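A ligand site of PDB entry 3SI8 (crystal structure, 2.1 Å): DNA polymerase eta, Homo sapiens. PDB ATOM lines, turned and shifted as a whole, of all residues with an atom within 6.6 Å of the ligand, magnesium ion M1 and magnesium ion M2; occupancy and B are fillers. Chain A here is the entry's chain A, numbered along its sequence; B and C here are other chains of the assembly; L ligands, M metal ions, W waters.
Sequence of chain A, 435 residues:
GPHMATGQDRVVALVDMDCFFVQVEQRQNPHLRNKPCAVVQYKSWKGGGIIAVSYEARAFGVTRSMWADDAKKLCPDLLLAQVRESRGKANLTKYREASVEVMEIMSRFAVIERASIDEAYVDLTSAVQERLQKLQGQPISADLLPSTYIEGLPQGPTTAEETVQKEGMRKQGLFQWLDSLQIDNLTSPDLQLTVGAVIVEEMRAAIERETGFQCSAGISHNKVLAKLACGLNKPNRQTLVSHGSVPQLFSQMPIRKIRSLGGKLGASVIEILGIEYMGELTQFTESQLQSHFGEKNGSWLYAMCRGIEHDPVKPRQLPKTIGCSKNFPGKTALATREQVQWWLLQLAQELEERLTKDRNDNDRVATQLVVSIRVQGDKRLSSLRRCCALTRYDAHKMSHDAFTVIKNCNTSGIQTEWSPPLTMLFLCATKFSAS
An oxygen (O4) of the ligand lies within salt-bridge range of the guanidinium group (NH1) of Arg 64 (3.4 Å). O9 of the ligand lies within salt-bridge range of NH1 of Arg 58 (3.4 Å). N of Cys 19 is in hydrogen-bond range of O6 of the ligand (3.0 Å). The backbone NH (N) of Phe 21 sits at hydrogen-bond distance from an oxygen (O7) of the ligand, 3.0 Å away. An oxygen (O6) of the ligand is in hydrogen-bond range of the side-chain hydroxyl of Tyr 55. An oxygen (O2) of the ligand lies close to the backbone NH (N) of Phe 20, at 3.2 Å. NZ of Lys 234 lies within salt-bridge range of O6 of the ligand (3.3 Å). O4 of TTD 5 of chain C is in hydrogen-bond range of a nitrogen (N3) of the ligand (2.9 Å).
The side-chain carboxylate (OD1) of Asp 16 lies close to the side-chain amino group (NZ) of Lys 234, at 3.4 Å. The guanidinium group (NH1) of Arg 58 lies within hydrogen-bond range of the side-chain hydroxyl (OH) of Tyr 55, 3.2 Å away. OG of Ser 116 lies close to N of Glu 119, 3.3 Å away. The side-chain carboxylate (OD1) of Asp 18 is in hydrogen-bond range of the side-chain hydroxyl (OG) of Ser 216. NZ of Lys 234 lies within salt-bridge range of OD1 of Asp 18 (3.3 Å). O2 of TTD 5 of chain C is in hydrogen-bond range of the side-chain amide nitrogen (NE2) of Gln 41, 2.6 Å away. The backbone NH of Asp 16 is in hydrogen-bond range of the backbone carbonyl oxygen of Ser 216, at 2.9 Å. N of Asp 118 sits close to OG of Ser 116.
Residues that only touch the ligand: Asp 18, Ile 51 and Ala 52. Of the 23 residues printed, 15 come within 4 Å of the ligand. The nearest printed residue that does not touch the ligand is Ile 117 (4.1 Å).
Of the 23 residues printed, 3 come within 4 Å of magnesium ion M1. Along chain A the residues within 4 Å of magnesium ion M1 span positions 16 to 118.
OG of Ser 116 touches magnesium ion M2, at 3.9 Å. Of the 23 residues printed, 5 come within 4 Å of magnesium ion M2. Along chain A the residues within 4 Å of magnesium ion M2 span positions 16 to 119. The nearest printed residue that does not touch magnesium ion M2 is Met 17 (5.5 Å).
Magnesium ion M1 is bound by OD1 of Asp 16 (2.1 Å), OD1 of Asp 118 (2.2 Å), O of Met 17 (2.2 Å), O3 of the ligand (2.3 Å), O1 of the ligand (2.4 Å) and O2 of the ligand (2.4 Å). Magnesium ion M1 has six donor atoms within binding distance.
Magnesium ion M2 is bound by OE2 of Glu 119 (2.0 Å), OD2 of Asp 16 (2.1 Å), water W1 (2.2 Å), O3' of DA 9 of chain B (2.2 Å), OD2 of Asp 118 (2.3 Å) and O1 of the ligand (2.4 Å). Magnesium ion M2 has six donor atoms within binding distance.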
ATOM      1  N   ASP A  16       9.867  36.508   5.681  1.00  0.00           N
ATOM      2  CA  ASP A  16       9.698  35.396   6.611  1.00  0.00           C
ATOM      3  C   ASP A  16      11.048  34.727   6.832  1.00  0.00           C
ATOM      4  O   ASP A  16      11.756  34.426   5.868  1.00  0.00           O
ATOM      5  CB  ASP A  16       8.684  34.396   6.048  1.00  0.00           C
ATOM      6  CG  ASP A  16       8.506  33.182   6.941  1.00  0.00           C
ATOM      7  OD1 ASP A  16       9.434  32.344   6.991  1.00  0.00           O
ATOM      8  OD2 ASP A  16       7.438  33.053   7.589  1.00  0.00           O
ATOM      9  N   MET A  17      11.384  34.532   8.101  1.00  0.00           N
ATOM     10  CA  MET A  17      12.641  33.885   8.487  1.00  0.00           C
ATOM     11  C   MET A  17      12.659  32.412   8.043  1.00  0.00           C
ATOM     12  O   MET A  17      11.632  31.709   8.138  1.00  0.00           O
ATOM     13  CB  MET A  17      12.819  33.931  10.010  1.00  0.00           C
ATOM     14  CG  MET A  17      12.667  35.303  10.601  1.00  0.00           C
ATOM     15  SD  MET A  17      14.022  36.367  10.095  1.00  0.00           S
ATOM     16  CE  MET A  17      13.294  37.290   8.851  1.00  0.00           C
ATOM     17  N   ASP A  18      13.811  31.969   7.576  1.00  0.00           N
ATOM     18  CA  ASP A  18      14.001  30.582   7.137  1.00  0.00           C
ATOM     19  C   ASP A  18      14.129  29.679   8.377  1.00  0.00           C
ATOM     20  O   ASP A  18      14.869  30.019   9.314  1.00  0.00           O
ATOM     21  CB  ASP A  18      15.262  30.482   6.252  1.00  0.00           C
ATOM     22  CG  ASP A  18      15.180  31.356   4.990  1.00  0.00           C
ATOM     23  OD1 ASP A  18      14.085  31.423   4.376  1.00  0.00           O
ATOM     24  OD2 ASP A  18      16.194  31.971   4.588  1.00  0.00           O
ATOM     25  N   CYS A  19      13.393  28.563   8.395  1.00  0.00           N
ATOM     26  CA  CYS A  19      13.435  27.613   9.517  1.00  0.00           C
ATOM     27  C   CYS A  19      13.839  28.361  10.786  1.00  0.00           C
ATOM     28  O   CYS A  19      14.866  28.072  11.402  1.00  0.00           O
ATOM     29  CB  CYS A  19      14.441  26.499   9.229  1.00  0.00           C
ATOM     30  SG  CYS A  19      16.091  27.094   8.805  1.00  0.00           S
ATOM     31  N   PHE A  20      13.009  29.314  11.161  1.00  0.00           N
ATOM     32  CA  PHE A  20      13.259  30.183  12.299  1.00  0.00           C
ATOM     33  C   PHE A  20      13.727  29.553  13.591  1.00  0.00           C
ATOM     34  O   PHE A  20      14.775  29.922  14.100  1.00  0.00           O
ATOM     35  CB  PHE A  20      12.033  31.049  12.559  1.00  0.00           C
ATOM     36  CG  PHE A  20      12.262  32.115  13.585  1.00  0.00           C
ATOM     37  CD1 PHE A  20      13.359  32.970  13.467  1.00  0.00           C
ATOM     38  CD2 PHE A  20      11.380  32.303  14.643  1.00  0.00           C
ATOM     39  CE1 PHE A  20      13.558  33.993  14.400  1.00  0.00           C
ATOM     40  CE2 PHE A  20      11.578  33.316  15.576  1.00  0.00           C
ATOM     41  CZ  PHE A  20      12.672  34.160  15.446  1.00  0.00           C
ATOM     42  N   PHE A  21      12.944  28.641  14.164  1.00  0.00           N
ATOM     43  CA  PHE A  21      13.358  28.028  15.430  1.00  0.00           C
ATOM     44  C   PHE A  21      14.735  27.370  15.296  1.00  0.00           C
ATOM     45  O   PHE A  21      15.563  27.483  16.212  1.00  0.00           O
ATOM     46  CB  PHE A  21      12.314  27.004  15.909  1.00  0.00           C
ATOM     47  CG  PHE A  21      11.091  27.620  16.552  1.00  0.00           C
ATOM     48  CD1 PHE A  21      10.789  28.966  16.357  1.00  0.00           C
ATOM     49  CD2 PHE A  21      10.207  26.839  17.296  1.00  0.00           C
ATOM     50  CE1 PHE A  21       9.625  29.521  16.907  1.00  0.00           C
ATOM     51  CE2 PHE A  21       9.054  27.375  17.851  1.00  0.00           C
ATOM     52  CZ  PHE A  21       8.755  28.720  17.648  1.00  0.00           C
ATOM     53  N   VAL A  22      14.983  26.718  14.166  1.00  0.00           N
ATOM     54  CA  VAL A  22      16.261  26.055  13.940  1.00  0.00           C
ATOM     55  C   VAL A  22      17.385  27.075  13.957  1.00  0.00           C
ATOM     56  O   VAL A  22      18.419  26.856  14.576  1.00  0.00           O
ATOM     57  CB  VAL A  22      16.300  25.310  12.587  1.00  0.00           C
ATOM     58  CG1 VAL A  22      17.729  24.900  12.276  1.00  0.00           C
ATOM     59  CG2 VAL A  22      15.402  24.079  12.627  1.00  0.00           C
ATOM     60  N   GLN A  41       8.746  19.385  19.683  1.00  0.00           N
ATOM     61  CA  GLN A  41       8.008  19.960  20.797  1.00  0.00           C
ATOM     62  C   GLN A  41       8.594  19.434  22.113  1.00  0.00           C
ATOM     63  O   GLN A  41       9.404  18.501  22.117  1.00  0.00           O
ATOM     64  CB  GLN A  41       6.525  19.596  20.677  1.00  0.00           C
ATOM     65  CG  GLN A  41       5.591  20.360  21.604  1.00  0.00           C
ATOM     66  CD  GLN A  41       5.763  21.855  21.518  1.00  0.00           C
ATOM     67  OE1 GLN A  41       6.685  22.412  22.108  1.00  0.00           O
ATOM     68  NE2 GLN A  41       4.892  22.506  20.774  1.00  0.00           N
ATOM     69  N   ILE A  51       8.422  20.542  14.671  1.00  0.00           N
ATOM     70  CA  ILE A  51       7.829  21.823  14.280  1.00  0.00           C
ATOM     71  C   ILE A  51       8.737  22.620  13.347  1.00  0.00           C
ATOM     72  O   ILE A  51       8.242  23.372  12.508  1.00  0.00           O
ATOM     73  CB  ILE A  51       7.502  22.705  15.503  1.00  0.00           C
ATOM     74  CG1 ILE A  51       8.683  22.711  16.481  1.00  0.00           C
ATOM     75  CG2 ILE A  51       6.232  22.209  16.167  1.00  0.00           C
ATOM     76  CD1 ILE A  51       8.431  23.516  17.719  1.00  0.00           C
ATOM     77  N   ALA A  52      10.059  22.469  13.505  1.00  0.00           N
ATOM     78  CA  ALA A  52      11.016  23.190  12.663  1.00  0.00           C
ATOM     79  C   ALA A  52      12.155  22.294  12.149  1.00  0.00           C
ATOM     80  O   ALA A  52      12.877  21.669  12.920  1.00  0.00           O
ATOM     81  CB  ALA A  52      11.577  24.391  13.427  1.00  0.00           C
ATOM     82  N   VAL A  53      12.335  22.275  10.824  1.00  0.00           N
ATOM     83  CA  VAL A  53      13.355  21.452  10.184  1.00  0.00           C
ATOM     84  C   VAL A  53      14.353  22.275   9.361  1.00  0.00           C
ATOM     85  O   VAL A  53      13.949  23.132   8.576  1.00  0.00           O
ATOM     86  CB  VAL A  53      12.718  20.435   9.237  1.00  0.00           C
ATOM     87  CG1 VAL A  53      13.785  19.534   8.643  1.00  0.00           C
ATOM     88  CG2 VAL A  53      11.665  19.617   9.966  1.00  0.00           C
ATOM     89  N   TYR A  55      16.988  23.177   6.388  1.00  0.00           N
ATOM     90  CA  TYR A  55      16.895  22.866   4.965  1.00  0.00           C
ATOM     91  C   TYR A  55      17.772  21.684   4.560  1.00  0.00           C
ATOM     92  O   TYR A  55      17.384  20.877   3.699  1.00  0.00           O
ATOM     93  CB  TYR A  55      17.243  24.117   4.132  1.00  0.00           C
ATOM     94  CG  TYR A  55      16.064  25.055   4.015  1.00  0.00           C
ATOM     95  CD1 TYR A  55      15.176  24.956   2.947  1.00  0.00           C
ATOM     96  CD2 TYR A  55      15.796  26.002   4.998  1.00  0.00           C
ATOM     97  CE1 TYR A  55      14.038  25.756   2.873  1.00  0.00           C
ATOM     98  CE2 TYR A  55      14.676  26.803   4.933  1.00  0.00           C
ATOM     99  CZ  TYR A  55      13.793  26.675   3.879  1.00  0.00           C
ATOM    100  OH  TYR A  55      12.679  27.467   3.850  1.00  0.00           O
ATOM    101  N   ARG A  58      15.691  18.825   5.107  1.00  0.00           N
ATOM    102  CA  ARG A  58      14.501  18.692   4.270  1.00  0.00           C
ATOM    103  C   ARG A  58      14.831  17.860   3.037  1.00  0.00           C
ATOM    104  O   ARG A  58      13.946  17.254   2.444  1.00  0.00           O
ATOM    105  CB  ARG A  58      13.985  20.075   3.849  1.00  0.00           C
ATOM    106  CG  ARG A  58      13.507  20.910   5.020  1.00  0.00           C
ATOM    107  CD  ARG A  58      12.939  22.251   4.618  1.00  0.00           C
ATOM    108  NE  ARG A  58      12.716  23.086   5.792  1.00  0.00           N
ATOM    109  CZ  ARG A  58      12.029  24.223   5.790  1.00  0.00           C
ATOM    110  NH1 ARG A  58      11.470  24.675   4.678  1.00  0.00           N
ATOM    111  NH2 ARG A  58      11.900  24.900   6.923  1.00  0.00           N
ATOM    112  N   ARG A  64       7.777  18.745   9.231  1.00  0.00           N
ATOM    113  CA  ARG A  64       7.225  19.021  10.562  1.00  0.00           C
ATOM    114  C   ARG A  64       5.914  18.237  10.608  1.00  0.00           C
ATOM    115  O   ARG A  64       5.389  17.852   9.576  1.00  0.00           O
ATOM    116  CB  ARG A  64       6.939  20.508  10.730  1.00  0.00           C
ATOM    117  CG  ARG A  64       5.804  21.016   9.859  1.00  0.00           C
ATOM    118  CD  ARG A  64       5.568  22.494  10.040  1.00  0.00           C
ATOM    119  NE  ARG A  64       4.482  22.985   9.182  1.00  0.00           N
ATOM    120  CZ  ARG A  64       4.152  24.262   9.052  1.00  0.00           C
ATOM    121  NH1 ARG A  64       4.811  25.193   9.733  1.00  0.00           N
ATOM    122  NH2 ARG A  64       3.161  24.617   8.242  1.00  0.00           N
ATOM    123  N   SER A 116       3.232  37.279  12.304  1.00  0.00           N
ATOM    124  CA  SER A 116       3.451  36.055  13.068  1.00  0.00           C
ATOM    125  C   SER A 116       4.773  36.209  13.791  1.00  0.00           C
ATOM    126  O   SER A 116       5.421  37.249  13.663  1.00  0.00           O
ATOM    127  CB  SER A 116       3.511  34.832  12.152  1.00  0.00           C
ATOM    128  OG  SER A 116       4.798  34.710  11.580  1.00  0.00           O
ATOM    129  N   ILE A 117       5.186  35.171  14.504  1.00  0.00           N
ATOM    130  CA  ILE A 117       6.440  35.244  15.238  1.00  0.00           C
ATOM    131  C   ILE A 117       7.683  35.403  14.364  1.00  0.00           C
ATOM    132  O   ILE A 117       8.705  35.900  14.825  1.00  0.00           O
ATOM    133  CB  ILE A 117       6.625  34.003  16.142  1.00  0.00           C
ATOM    134  CG1 ILE A 117       7.726  34.268  17.168  1.00  0.00           C
ATOM    135  CG2 ILE A 117       6.975  32.791  15.290  1.00  0.00           C
ATOM    136  CD1 ILE A 117       7.863  33.169  18.225  1.00  0.00           C
ATOM    137  N   ASP A 118       7.613  34.996  13.087  1.00  0.00           N
ATOM    138  CA  ASP A 118       8.795  35.124  12.228  1.00  0.00           C
ATOM    139  C   ASP A 118       8.554  35.791  10.879  1.00  0.00           C
ATOM    140  O   ASP A 118       9.356  35.633   9.959  1.00  0.00           O
ATOM    141  CB  ASP A 118       9.412  33.756  11.942  1.00  0.00           C
ATOM    142  CG  ASP A 118       8.749  33.052  10.790  1.00  0.00           C
ATOM    143  OD1 ASP A 118       9.438  32.306  10.065  1.00  0.00           O
ATOM    144  OD2 ASP A 118       7.531  33.267  10.616  1.00  0.00           O
ATOM    145  N   GLU A 119       7.458  36.531  10.748  1.00  0.00           N
ATOM    146  CA  GLU A 119       7.177  37.208   9.479  1.00  0.00           C
ATOM    147  C   GLU A 119       6.401  38.497   9.644  1.00  0.00           C
ATOM    148  O   GLU A 119       5.630  38.656  10.590  1.00  0.00           O
ATOM    149  CB  GLU A 119       6.430  36.277   8.545  1.00  0.00           C
ATOM    150  CG  GLU A 119       5.031  35.962   9.022  1.00  0.00           C
ATOM    151  CD  GLU A 119       4.514  34.668   8.448  1.00  0.00           C
ATOM    152  OE1 GLU A 119       3.627  34.724   7.568  1.00  0.00           O
ATOM    153  OE2 GLU A 119       4.997  33.594   8.862  1.00  0.00           O
ATOM    154  N   SER A 216      13.698  35.005   3.706  1.00  0.00           N
ATOM    155  CA  SER A 216      13.209  35.172   2.341  1.00  0.00           C
ATOM    156  C   SER A 216      12.160  36.267   2.330  1.00  0.00           C
ATOM    157  O   SER A 216      11.629  36.677   3.379  1.00  0.00           O
ATOM    158  CB  SER A 216      12.608  33.868   1.849  1.00  0.00           C
ATOM    159  OG  SER A 216      13.587  32.840   1.859  1.00  0.00           O
ATOM    160  N   LYS A 234      12.830  29.738  -1.675  1.00  0.00           N
ATOM    161  CA  LYS A 234      13.428  29.633  -0.358  1.00  0.00           C
ATOM    162  C   LYS A 234      14.567  28.627  -0.493  1.00  0.00           C
ATOM    163  O   LYS A 234      14.483  27.702  -1.304  1.00  0.00           O
ATOM    164  CB  LYS A 234      12.427  29.095   0.650  1.00  0.00           C
ATOM    165  CG  LYS A 234      11.540  30.124   1.319  1.00  0.00           C
ATOM    166  CD  LYS A 234      10.539  29.402   2.206  1.00  0.00           C
ATOM    167  CE  LYS A 234       9.877  30.337   3.198  1.00  0.00           C
ATOM    168  NZ  LYS A 234      10.867  30.987   4.165  1.00  0.00           N
ATOM    169  N   PRO A 235      15.621  28.765   0.322  1.00  0.00           N
ATOM    170  CA  PRO A 235      15.798  29.799   1.344  1.00  0.00           C
ATOM    171  C   PRO A 235      16.767  30.912   0.939  1.00  0.00           C
ATOM    172  O   PRO A 235      17.413  30.847  -0.103  1.00  0.00           O
ATOM    173  CB  PRO A 235      16.355  28.998   2.515  1.00  0.00           C
ATOM    174  CG  PRO A 235      17.340  28.112   1.792  1.00  0.00           C
ATOM    175  CD  PRO A 235      16.521  27.631   0.573  1.00  0.00           C
ATOM    176  P    DA B   9       0.659  30.118   7.154  1.00  0.00           P
ATOM    177  OP1  DA B   9       0.958  30.876   5.923  1.00  0.00           O
ATOM    178  OP2  DA B   9       0.449  28.658   7.088  1.00  0.00           O
ATOM    179  O5'  DA B   9       1.791  30.435   8.227  1.00  0.00           O
ATOM    180  C5'  DA B   9       1.797  31.665   8.941  1.00  0.00           C
ATOM    181  C4'  DA B   9       2.491  31.494  10.273  1.00  0.00           C
ATOM    182  O4'  DA B   9       1.590  30.909  11.241  1.00  0.00           O
ATOM    183  C3'  DA B   9       3.694  30.562  10.180  1.00  0.00           C
ATOM    184  O3'  DA B   9       4.889  31.214  10.591  1.00  0.00           O
ATOM    185  C2'  DA B   9       3.270  29.306  10.920  1.00  0.00           C
ATOM    186  C1'  DA B   9       2.188  29.795  11.878  1.00  0.00           C
ATOM    187  N9   DA B   9       1.136  28.825  12.142  1.00  0.00           N
ATOM    188  C8   DA B   9       0.278  28.281  11.215  1.00  0.00           C
ATOM    189  N7   DA B   9      -0.593  27.444  11.733  1.00  0.00           N
ATOM    190  C5   DA B   9      -0.284  27.420  13.087  1.00  0.00           C
ATOM    191  C6   DA B   9      -0.836  26.710  14.171  1.00  0.00           C
ATOM    192  N6   DA B   9      -1.873  25.870  14.050  1.00  0.00           N
ATOM    193  N1   DA B   9      -0.284  26.901  15.396  1.00  0.00           N
ATOM    194  C2   DA B   9       0.739  27.759  15.498  1.00  0.00           C
ATOM    195  N3   DA B   9       1.346  28.476  14.552  1.00  0.00           N
ATOM    196  C4   DA B   9       0.782  28.265  13.354  1.00  0.00           C
ATOM    197  P   TTD C   5       2.227  15.701  21.253  1.00  0.00           P
ATOM    198  OP1 TTD C   5       1.814  14.527  22.053  1.00  0.00           O
ATOM    199  OP2 TTD C   5       3.668  16.078  21.163  1.00  0.00           O
ATOM    200  O5' TTD C   5       1.433  16.969  21.776  1.00  0.00           O
ATOM    201  C5' TTD C   5       1.338  18.095  20.928  1.00  0.00           C
ATOM    202  C4R TTD C   5       1.831  19.332  21.647  1.00  0.00           C
ATOM    203  O4' TTD C   5       2.079  20.304  20.612  1.00  0.00           O
ATOM    204  C3R TTD C   5       0.767  19.960  22.534  1.00  0.00           C
ATOM    205  O3R TTD C   5       1.380  20.670  23.606  1.00  0.00           O
ATOM    206  C2' TTD C   5       0.067  20.922  21.593  1.00  0.00           C
ATOM    207  C1' TTD C   5       1.237  21.430  20.768  1.00  0.00           C
ATOM    208  N1  TTD C   5       0.858  21.923  19.443  1.00  0.00           N
ATOM    209  C2  TTD C   5       1.800  22.423  18.607  1.00  0.00           C
ATOM    210  O2  TTD C   5       2.940  22.562  18.996  1.00  0.00           O
ATOM    211  N3  TTD C   5       1.452  22.838  17.342  1.00  0.00           N
ATOM    212  C4  TTD C   5       0.187  22.740  16.769  1.00  0.00           C
ATOM    213  O4  TTD C   5       0.054  23.024  15.577  1.00  0.00           O
ATOM    214  C5  TTD C   5      -0.958  22.280  17.516  1.00  0.00           C
ATOM    215  C5A TTD C   5      -1.596  21.098  16.793  1.00  0.00           C
ATOM    216  C6  TTD C   5      -0.499  21.943  18.935  1.00  0.00           C
ATOM    217  PB  TTD C   5       0.453  21.270  24.783  1.00  0.00           P
ATOM    218  O5P TTD C   5      -0.231  20.133  25.451  1.00  0.00           O
ATOM    219  O4P TTD C   5       1.316  22.181  25.575  1.00  0.00           O
ATOM    220  O5R TTD C   5      -0.652  22.102  24.001  1.00  0.00           O
ATOM    221  C5R TTD C   5      -0.730  23.513  24.094  1.00  0.00           C
ATOM    222  O4R TTD C   5       0.232  23.677  21.857  1.00  0.00           O
ATOM    223  C2R TTD C   5      -0.298  25.949  21.765  1.00  0.00           C
ATOM    224  C1R TTD C   5       0.204  24.763  20.943  1.00  0.00           C
ATOM    225  N1T TTD C   5      -0.485  24.524  19.617  1.00  0.00           N
ATOM    226  C2T TTD C   5      -0.479  25.530  18.687  1.00  0.00           C
ATOM    227  O2T TTD C   5       0.232  26.509  18.824  1.00  0.00           O
ATOM    228  N3T TTD C   5      -1.220  25.425  17.568  1.00  0.00           N
ATOM    229  C4T TTD C   5      -2.058  24.353  17.470  1.00  0.00           C
ATOM    230  O4T TTD C   5      -2.918  24.411  16.604  1.00  0.00           O
ATOM    231  C5T TTD C   5      -2.013  23.146  18.294  1.00  0.00           C
ATOM    232  C5M TTD C   5      -3.356  22.424  18.491  1.00  0.00           C
ATOM    233  C6T TTD C   5      -1.148  23.200  19.618  1.00  0.00           C
ATOM    234  C4' TTD C   5       0.327  24.157  23.235  1.00  0.00           C
ATOM    235  C3' TTD C   5       0.221  25.683  23.168  1.00  0.00           C
ATOM    236  O3' TTD C   5       1.493  26.254  23.428  1.00  0.00           O
HETATM  237  N1  LIG L   1       2.851  24.708  15.870  1.00  0.00           N
HETATM  238  C1  LIG L   1       3.837  25.133  16.660  1.00  0.00           C
HETATM  239  N2  LIG L   1       4.846  25.876  16.188  1.00  0.00           N
HETATM  240  C2  LIG L   1       4.921  26.204  14.886  1.00  0.00           C
HETATM  241  C3  LIG L   1       3.880  25.775  14.002  1.00  0.00           C
HETATM  242  C4  LIG L   1       2.811  24.992  14.556  1.00  0.00           C
HETATM  243  N3  LIG L   1       1.781  24.526  13.768  1.00  0.00           N
HETATM  244  N4  LIG L   1       4.161  26.243  12.788  1.00  0.00           N
HETATM  245  C5  LIG L   1       5.280  26.913  12.828  1.00  0.00           C
HETATM  246  N5  LIG L   1       5.788  26.944  14.111  1.00  0.00           N
HETATM  247  P1  LIG L   1       7.158  28.912   9.563  1.00  0.00           P
HETATM  248  P2  LIG L   1       9.906  27.787   9.292  1.00  0.00           P
HETATM  249  P3  LIG L   1      10.278  28.179   6.599  1.00  0.00           P
HETATM  250  C6  LIG L   1       7.006  27.578  14.567  1.00  0.00           C
HETATM  251  O1  LIG L   1       7.492  30.032   9.092  1.00  0.00           O
HETATM  252  O2  LIG L   1      10.269  28.930   9.648  1.00  0.00           O
HETATM  253  O3  LIG L   1       9.550  29.260   6.777  1.00  0.00           O
HETATM  254  C7  LIG L   1       8.214  26.754  14.019  1.00  0.00           C
HETATM  255  O4  LIG L   1       5.952  28.351   9.213  1.00  0.00           O
HETATM  256  O5  LIG L   1      10.270  26.911  10.113  1.00  0.00           O
HETATM  257  O6  LIG L   1      11.483  28.406   6.072  1.00  0.00           O
HETATM  258  C8  LIG L   1       8.981  27.615  13.050  1.00  0.00           C
HETATM  259  O7  LIG L   1      10.293  27.611  13.078  1.00  0.00           O
HETATM  260  N6  LIG L   1       8.263  27.800   9.257  1.00  0.00           N
HETATM  261  O8  LIG L   1      10.451  27.419   7.915  1.00  0.00           O
HETATM  262  O9  LIG L   1       9.640  27.344   5.750  1.00  0.00           O
HETATM  263  C9  LIG L   1       8.262  28.958  13.275  1.00  0.00           C
HETATM  264  O10 LIG L   1       7.174  28.823  14.102  1.00  0.00           O
HETATM  265  C10 LIG L   1       7.982  29.572  11.896  1.00  0.00           C
HETATM  266  O11 LIG L   1       6.999  29.027  11.087  1.00  0.00           O
HETATM  267 MG    MG M   1       9.587  30.855   8.394  1.00  0.00          MG
HETATM  268 MG    MG M   2       6.271  32.132   9.087  1.00  0.00          MG
HETATM  269  O   HOH W   1       5.339  31.145   7.394  1.00  0.00           O
HETATM  270  O   HOH W   2       6.969  29.811   5.599  1.00  0.00           O
